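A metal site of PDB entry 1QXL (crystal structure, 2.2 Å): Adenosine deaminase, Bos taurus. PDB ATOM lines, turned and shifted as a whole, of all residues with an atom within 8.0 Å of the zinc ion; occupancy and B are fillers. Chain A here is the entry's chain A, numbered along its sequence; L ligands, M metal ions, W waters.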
ATOM      1  N   HIS A  14      13.755  23.429  21.549  1.00  0.00           N
ATOM      2  CA  HIS A  14      14.811  23.855  22.501  1.00  0.00           C
ATOM      3  C   HIS A  14      15.669  22.715  23.037  1.00  0.00           C
ATOM      4  O   HIS A  14      15.373  22.061  24.033  1.00  0.00           O
ATOM      5  CB  HIS A  14      14.250  24.641  23.728  1.00  0.00           C
ATOM      6  CG  HIS A  14      15.336  25.320  24.543  1.00  0.00           C
ATOM      7  ND1 HIS A  14      15.338  26.611  24.833  1.00  0.00           N
ATOM      8  CD2 HIS A  14      16.414  24.807  25.234  1.00  0.00           C
ATOM      9  CE1 HIS A  14      16.353  26.934  25.657  1.00  0.00           C
ATOM     10  NE2 HIS A  14      17.059  25.794  25.939  1.00  0.00           N
ATOM     11  N   VAL A  15      16.793  22.540  22.348  1.00  0.00           N
ATOM     12  CA  VAL A  15      17.725  21.434  22.654  1.00  0.00           C
ATOM     13  C   VAL A  15      19.107  21.850  22.158  1.00  0.00           C
ATOM     14  O   VAL A  15      19.294  22.266  21.028  1.00  0.00           O
ATOM     15  CB  VAL A  15      17.566  20.193  21.833  1.00  0.00           C
ATOM     16  CG1 VAL A  15      17.840  18.883  22.534  1.00  0.00           C
ATOM     17  CG2 VAL A  15      16.733  20.334  20.574  1.00  0.00           C
ATOM     18  N   HIS A  16      20.064  21.733  23.045  1.00  0.00           N
ATOM     19  CA  HIS A  16      21.470  22.013  22.682  1.00  0.00           C
ATOM     20  C   HIS A  16      22.256  20.816  22.094  1.00  0.00           C
ATOM     21  O   HIS A  16      22.459  19.802  22.745  1.00  0.00           O
ATOM     22  CB  HIS A  16      22.215  22.481  23.971  1.00  0.00           C
ATOM     23  CG  HIS A  16      21.658  23.797  24.585  1.00  0.00           C
ATOM     24  ND1 HIS A  16      22.174  25.020  24.407  1.00  0.00           N
ATOM     25  CD2 HIS A  16      20.567  23.965  25.435  1.00  0.00           C
ATOM     26  CE1 HIS A  16      21.466  25.938  25.112  1.00  0.00           C
ATOM     27  NE2 HIS A  16      20.439  25.307  25.759  1.00  0.00           N
ATOM     28  N   ARG A 100      20.201  24.004  18.665  1.00  0.00           N
ATOM     29  CA  ARG A 100      21.029  25.175  18.966  1.00  0.00           C
ATOM     30  C   ARG A 100      22.395  24.843  19.547  1.00  0.00           C
ATOM     31  O   ARG A 100      22.625  23.814  20.211  1.00  0.00           O
ATOM     32  CB  ARG A 100      20.222  26.020  19.922  1.00  0.00           C
ATOM     33  CG  ARG A 100      20.256  25.576  21.385  1.00  0.00           C
ATOM     34  CD  ARG A 100      19.385  26.489  22.214  1.00  0.00           C
ATOM     35  NE  ARG A 100      18.086  26.532  21.578  1.00  0.00           N
ATOM     36  CZ  ARG A 100      17.112  27.381  21.869  1.00  0.00           C
ATOM     37  NH1 ARG A 100      17.320  28.389  22.684  1.00  0.00           N
ATOM     38  NH2 ARG A 100      15.895  27.203  21.395  1.00  0.00           N
ATOM     39  N   CYS A 152      24.074  30.032  18.893  1.00  0.00           N
ATOM     40  CA  CYS A 152      23.924  30.693  20.174  1.00  0.00           C
ATOM     41  C   CYS A 152      24.946  31.784  20.293  1.00  0.00           C
ATOM     42  O   CYS A 152      26.131  31.485  20.218  1.00  0.00           O
ATOM     43  CB  CYS A 152      24.248  29.743  21.335  1.00  0.00           C
ATOM     44  SG  CYS A 152      22.940  28.505  21.462  1.00  0.00           S
ATOM     45  N   ASP A 180      20.312  32.953  19.134  1.00  0.00           N
ATOM     46  CA  ASP A 180      19.921  32.714  20.504  1.00  0.00           C
ATOM     47  C   ASP A 180      20.921  33.406  21.397  1.00  0.00           C
ATOM     48  O   ASP A 180      22.016  33.706  20.953  1.00  0.00           O
ATOM     49  CB  ASP A 180      19.936  31.187  20.811  1.00  0.00           C
ATOM     50  CG  ASP A 180      19.549  30.735  22.207  1.00  0.00           C
ATOM     51  OD1 ASP A 180      20.099  29.731  22.607  1.00  0.00           O
ATOM     52  OD2 ASP A 180      18.711  31.339  22.893  1.00  0.00           O
ATOM     53  N   LEU A 181      20.549  33.609  22.670  1.00  0.00           N
ATOM     54  CA  LEU A 181      21.547  33.981  23.678  1.00  0.00           C
ATOM     55  C   LEU A 181      21.453  33.071  24.844  1.00  0.00           C
ATOM     56  O   LEU A 181      20.435  32.890  25.487  1.00  0.00           O
ATOM     57  CB  LEU A 181      21.235  35.414  24.099  1.00  0.00           C
ATOM     58  CG  LEU A 181      22.182  36.469  24.652  1.00  0.00           C
ATOM     59  CD1 LEU A 181      21.363  37.121  25.723  1.00  0.00           C
ATOM     60  CD2 LEU A 181      23.712  36.222  24.697  1.00  0.00           C
ATOM     61  N   ALA A 182      22.554  32.400  25.045  1.00  0.00           N
ATOM     62  CA  ALA A 182      22.680  31.438  26.126  1.00  0.00           C
ATOM     63  C   ALA A 182      23.851  31.841  27.052  1.00  0.00           C
ATOM     64  O   ALA A 182      24.675  32.688  26.797  1.00  0.00           O
ATOM     65  CB  ALA A 182      22.993  30.027  25.562  1.00  0.00           C
ATOM     66  N   GLY A 183      23.846  31.120  28.170  1.00  0.00           N
ATOM     67  CA  GLY A 183      24.923  31.030  29.158  1.00  0.00           C
ATOM     68  C   GLY A 183      24.782  31.865  30.399  1.00  0.00           C
ATOM     69  O   GLY A 183      25.664  32.655  30.609  1.00  0.00           O
ATOM     70  N   HIS A 213      17.574  32.904  25.990  1.00  0.00           N
ATOM     71  CA  HIS A 213      17.267  32.240  27.239  1.00  0.00           C
ATOM     72  C   HIS A 213      17.066  33.248  28.364  1.00  0.00           C
ATOM     73  O   HIS A 213      17.932  34.079  28.603  1.00  0.00           O
ATOM     74  CB  HIS A 213      18.434  31.396  27.702  1.00  0.00           C
ATOM     75  CG  HIS A 213      18.789  30.140  26.927  1.00  0.00           C
ATOM     76  ND1 HIS A 213      19.287  30.101  25.731  1.00  0.00           N
ATOM     77  CD2 HIS A 213      18.745  28.841  27.398  1.00  0.00           C
ATOM     78  CE1 HIS A 213      19.553  28.832  25.413  1.00  0.00           C
ATOM     79  NE2 HIS A 213      19.227  28.025  26.446  1.00  0.00           N
ATOM     80  N   GLU A 216      15.167  31.536  33.344  1.00  0.00           N
ATOM     81  CA  GLU A 216      15.390  30.204  33.902  1.00  0.00           C
ATOM     82  C   GLU A 216      15.809  30.257  35.384  1.00  0.00           C
ATOM     83  O   GLU A 216      15.227  29.652  36.274  1.00  0.00           O
ATOM     84  CB  GLU A 216      16.426  29.391  33.091  1.00  0.00           C
ATOM     85  CG  GLU A 216      16.805  27.951  33.542  1.00  0.00           C
ATOM     86  CD  GLU A 216      17.966  27.422  32.717  1.00  0.00           C
ATOM     87  OE1 GLU A 216      18.556  28.184  31.947  1.00  0.00           O
ATOM     88  OE2 GLU A 216      18.279  26.237  32.800  1.00  0.00           O
ATOM     89  N   GLY A 236      13.486  31.186  25.805  1.00  0.00           N
ATOM     90  CA  GLY A 236      13.974  30.033  26.543  1.00  0.00           C
ATOM     91  C   GLY A 236      13.694  30.019  28.026  1.00  0.00           C
ATOM     92  O   GLY A 236      14.214  30.834  28.789  1.00  0.00           O
ATOM     93  N   HIS A 237      12.823  29.028  28.350  1.00  0.00           N
ATOM     94  CA  HIS A 237      12.235  28.837  29.646  1.00  0.00           C
ATOM     95  C   HIS A 237      11.159  29.904  30.038  1.00  0.00           C
ATOM     96  O   HIS A 237       9.946  29.727  30.014  1.00  0.00           O
ATOM     97  CB  HIS A 237      13.332  28.824  30.741  1.00  0.00           C
ATOM     98  CG  HIS A 237      14.410  27.791  30.484  1.00  0.00           C
ATOM     99  ND1 HIS A 237      14.320  26.491  30.842  1.00  0.00           N
ATOM    100  CD2 HIS A 237      15.670  27.970  29.907  1.00  0.00           C
ATOM    101  CE1 HIS A 237      15.453  25.834  30.527  1.00  0.00           C
ATOM    102  NE2 HIS A 237      16.278  26.751  29.943  1.00  0.00           N
ATOM    103  N   GLU A 259       9.528  28.206  25.652  1.00  0.00           N
ATOM    104  CA  GLU A 259      10.134  26.913  25.402  1.00  0.00           C
ATOM    105  C   GLU A 259      10.437  26.216  26.717  1.00  0.00           C
ATOM    106  O   GLU A 259      11.485  26.383  27.304  1.00  0.00           O
ATOM    107  CB  GLU A 259      11.434  27.101  24.574  1.00  0.00           C
ATOM    108  CG  GLU A 259      11.362  28.121  23.399  1.00  0.00           C
ATOM    109  CD  GLU A 259      12.716  28.495  22.815  1.00  0.00           C
ATOM    110  OE1 GLU A 259      12.746  29.070  21.743  1.00  0.00           O
ATOM    111  OE2 GLU A 259      13.748  28.205  23.395  1.00  0.00           O
ATOM    112  N   CYS A 261      11.346  23.491  29.618  1.00  0.00           N
ATOM    113  CA  CYS A 261      12.164  22.322  29.834  1.00  0.00           C
ATOM    114  C   CYS A 261      11.888  21.678  31.201  1.00  0.00           C
ATOM    115  O   CYS A 261      12.617  21.853  32.134  1.00  0.00           O
ATOM    116  CB  CYS A 261      13.636  22.563  29.578  1.00  0.00           C
ATOM    117  SG  CYS A 261      13.909  23.554  28.083  1.00  0.00           S
ATOM    118  N   SER A 264      14.791  19.196  32.767  1.00  0.00           N
ATOM    119  CA  SER A 264      15.798  20.251  32.954  1.00  0.00           C
ATOM    120  C   SER A 264      15.604  21.154  34.184  1.00  0.00           C
ATOM    121  O   SER A 264      16.476  21.328  35.035  1.00  0.00           O
ATOM    122  CB  SER A 264      15.946  21.068  31.721  1.00  0.00           C
ATOM    123  OG  SER A 264      16.962  22.046  31.858  1.00  0.00           O
ATOM    124  N   ASN A 292      10.382  20.394  25.944  1.00  0.00           N
ATOM    125  CA  ASN A 292      11.687  20.320  25.329  1.00  0.00           C
ATOM    126  C   ASN A 292      12.631  19.659  26.299  1.00  0.00           C
ATOM    127  O   ASN A 292      12.438  19.695  27.506  1.00  0.00           O
ATOM    128  CB  ASN A 292      12.273  21.704  25.151  1.00  0.00           C
ATOM    129  CG  ASN A 292      11.455  22.477  24.170  1.00  0.00           C
ATOM    130  OD1 ASN A 292      11.681  22.386  22.968  1.00  0.00           O
ATOM    131  ND2 ASN A 292      10.460  23.196  24.691  1.00  0.00           N
ATOM    132  N   THR A 293      13.684  19.059  25.746  1.00  0.00           N
ATOM    133  CA  THR A 293      14.503  18.487  26.788  1.00  0.00           C
ATOM    134  C   THR A 293      15.807  19.118  27.055  1.00  0.00           C
ATOM    135  O   THR A 293      16.464  18.740  28.007  1.00  0.00           O
ATOM    136  CB  THR A 293      14.792  16.990  26.652  1.00  0.00           C
ATOM    137  OG1 THR A 293      15.191  16.387  28.029  1.00  0.00           O
ATOM    138  CG2 THR A 293      15.733  16.904  25.413  1.00  0.00           C
ATOM    139  N   ASP A 294      16.178  20.094  26.196  1.00  0.00           N
ATOM    140  CA  ASP A 294      17.357  20.922  26.562  1.00  0.00           C
ATOM    141  C   ASP A 294      18.743  20.304  26.428  1.00  0.00           C
ATOM    142  O   ASP A 294      19.515  20.662  25.542  1.00  0.00           O
ATOM    143  CB  ASP A 294      17.120  21.581  27.930  1.00  0.00           C
ATOM    144  CG  ASP A 294      17.857  22.861  28.255  1.00  0.00           C
ATOM    145  OD1 ASP A 294      18.403  23.465  27.368  1.00  0.00           O
ATOM    146  OD2 ASP A 294      17.854  23.303  29.409  1.00  0.00           O
ATOM    147  N   ASP A 295      19.022  19.371  27.347  1.00  0.00           N
ATOM    148  CA  ASP A 295      20.319  18.681  27.290  1.00  0.00           C
ATOM    149  C   ASP A 295      20.205  17.206  27.686  1.00  0.00           C
ATOM    150  O   ASP A 295      20.526  16.838  28.808  1.00  0.00           O
ATOM    151  CB  ASP A 295      21.351  19.240  28.312  1.00  0.00           C
ATOM    152  CG  ASP A 295      21.601  20.758  28.199  1.00  0.00           C
ATOM    153  OD1 ASP A 295      22.529  21.117  27.453  1.00  0.00           O
ATOM    154  OD2 ASP A 295      20.867  21.500  28.888  1.00  0.00           O
ATOM    155  N   PHE A 299      21.239  15.692  31.316  1.00  0.00           N
ATOM    156  CA  PHE A 299      20.144  15.323  32.229  1.00  0.00           C
ATOM    157  C   PHE A 299      19.694  13.866  32.235  1.00  0.00           C
ATOM    158  O   PHE A 299      18.743  13.528  32.925  1.00  0.00           O
ATOM    159  CB  PHE A 299      18.943  16.258  31.979  1.00  0.00           C
ATOM    160  CG  PHE A 299      19.303  17.736  32.030  1.00  0.00           C
ATOM    161  CD1 PHE A 299      20.101  18.226  33.090  1.00  0.00           C
ATOM    162  CD2 PHE A 299      18.840  18.599  31.010  1.00  0.00           C
ATOM    163  CE1 PHE A 299      20.423  19.604  33.123  1.00  0.00           C
ATOM    164  CE2 PHE A 299      19.193  19.981  31.033  1.00  0.00           C
ATOM    165  CZ  PHE A 299      19.975  20.458  32.101  1.00  0.00           C
HETATM  166  C1  LIG L   1      24.348  25.721  27.530  1.00  0.00           C
HETATM  167  N1  LIG L   1      25.031  24.951  26.490  1.00  0.00           N
HETATM  168  C2  LIG L   1      24.507  23.727  26.469  1.00  0.00           C
HETATM  169  N2  LIG L   1      23.497  23.621  27.339  1.00  0.00           N
HETATM  170  C3  LIG L   1      23.452  24.894  28.072  1.00  0.00           C
HETATM  171  C4  LIG L   1      22.569  25.192  29.230  1.00  0.00           C
HETATM  172  O1  LIG L   1      22.670  26.241  29.850  1.00  0.00           O
HETATM  173  N3  LIG L   1      21.645  24.321  29.548  1.00  0.00           N
HETATM  174  C5  LIG L   1      26.159  25.410  25.706  1.00  0.00           C
HETATM  175  C6  LIG L   1      25.723  25.983  24.322  1.00  0.00           C
HETATM  176  O2  LIG L   1      24.680  25.104  23.725  1.00  0.00           O
HETATM  177  C7  LIG L   1      26.992  26.416  26.532  1.00  0.00           C
HETATM  178  C8  LIG L   1      27.843  25.743  27.645  1.00  0.00           C
HETATM  179  N4  LIG L   1      28.469  26.846  28.438  1.00  0.00           N
HETATM  180  C9  LIG L   1      29.748  27.316  28.337  1.00  0.00           C
HETATM  181  C10 LIG L   1      29.928  28.368  29.234  1.00  0.00           C
HETATM  182  C11 LIG L   1      28.682  28.549  29.933  1.00  0.00           C
HETATM  183  C12 LIG L   1      27.796  27.554  29.418  1.00  0.00           C
HETATM  184  C13 LIG L   1      28.265  29.411  30.902  1.00  0.00           C
HETATM  185  C14 LIG L   1      26.968  29.332  31.384  1.00  0.00           C
HETATM  186  C15 LIG L   1      26.082  28.347  30.872  1.00  0.00           C
HETATM  187  C16 LIG L   1      26.528  27.465  29.899  1.00  0.00           C
HETATM  188  N5  LIG L   1      24.783  28.210  31.225  1.00  0.00           N
HETATM  189  C17 LIG L   1      24.229  28.753  32.301  1.00  0.00           C
HETATM  190  O3  LIG L   1      24.710  29.589  33.036  1.00  0.00           O
HETATM  191  C18 LIG L   1      22.854  28.196  32.548  1.00  0.00           C
HETATM  192  C19 LIG L   1      22.747  27.555  33.935  1.00  0.00           C
HETATM  193  C20 LIG L   1      21.927  26.973  37.232  1.00  0.00           C
HETATM  194  C21 LIG L   1      21.900  25.933  36.304  1.00  0.00           C
HETATM  195  C22 LIG L   1      22.580  24.761  36.556  1.00  0.00           C
HETATM  196  C23 LIG L   1      23.180  24.589  37.785  1.00  0.00           C
HETATM  197  C24 LIG L   1      23.154  25.609  38.736  1.00  0.00           C
HETATM  198  C25 LIG L   1      22.549  26.821  38.463  1.00  0.00           C
HETATM  199  C26 LIG L   1      21.984  26.257  33.859  1.00  0.00           C
HETATM  200  C27 LIG L   1      21.105  26.063  35.075  1.00  0.00           C
HETATM  201 ZN    ZN M   1      18.870  25.807  26.800  1.00  0.00          ZN
HETATM  202  O   HOH W   1      18.657  25.711  28.784  1.00  0.00           O
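N2 of the ligand is in hydrogen-bond range of OD1 of Asp 295, at 2.7 Å. A ring nitrogen (ND1) of His 16 sits at hydrogen-bond distance from an oxygen (O2) of the ligand, 2.6 Å away.
ND1 of His 14 lies within hydrogen-bond range of NH1 of Arg 100, 3.4 Å away. OG of Ser 264 sits at hydrogen-bond distance from OD2 of Asp 294 (2.9 Å). ND1 of His 14 is in hydrogen-bond range of OE2 of Glu 259, at 2.7 Å. N of His 213 is in hydrogen-bond range of O of Leu 181. ND1 of His 213 is in hydrogen-bond range of OD2 of Asp 180. The backbone NH (N) of His 14 is in hydrogen-bond range of the side-chain amide oxygen (OD1) of Asn 292 (2.7 Å).
Four residues have an atom within 4 Å of the zinc ion: His 14, His 16, His 213 and Asp 294.
The zinc ion is bound by NE2 of His 16, water W1, NE2 of His 14, NE2 of His 213 and OD1 of Asp 294.
Water W1 lies within hydrogen-bond range of the side-chain carboxylate of Asp 294 (2.6 Å), a ring nitrogen (NE2) of His 237 (2.8 Å) and a nitrogen (N3) of the ligand (3.4 Å).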
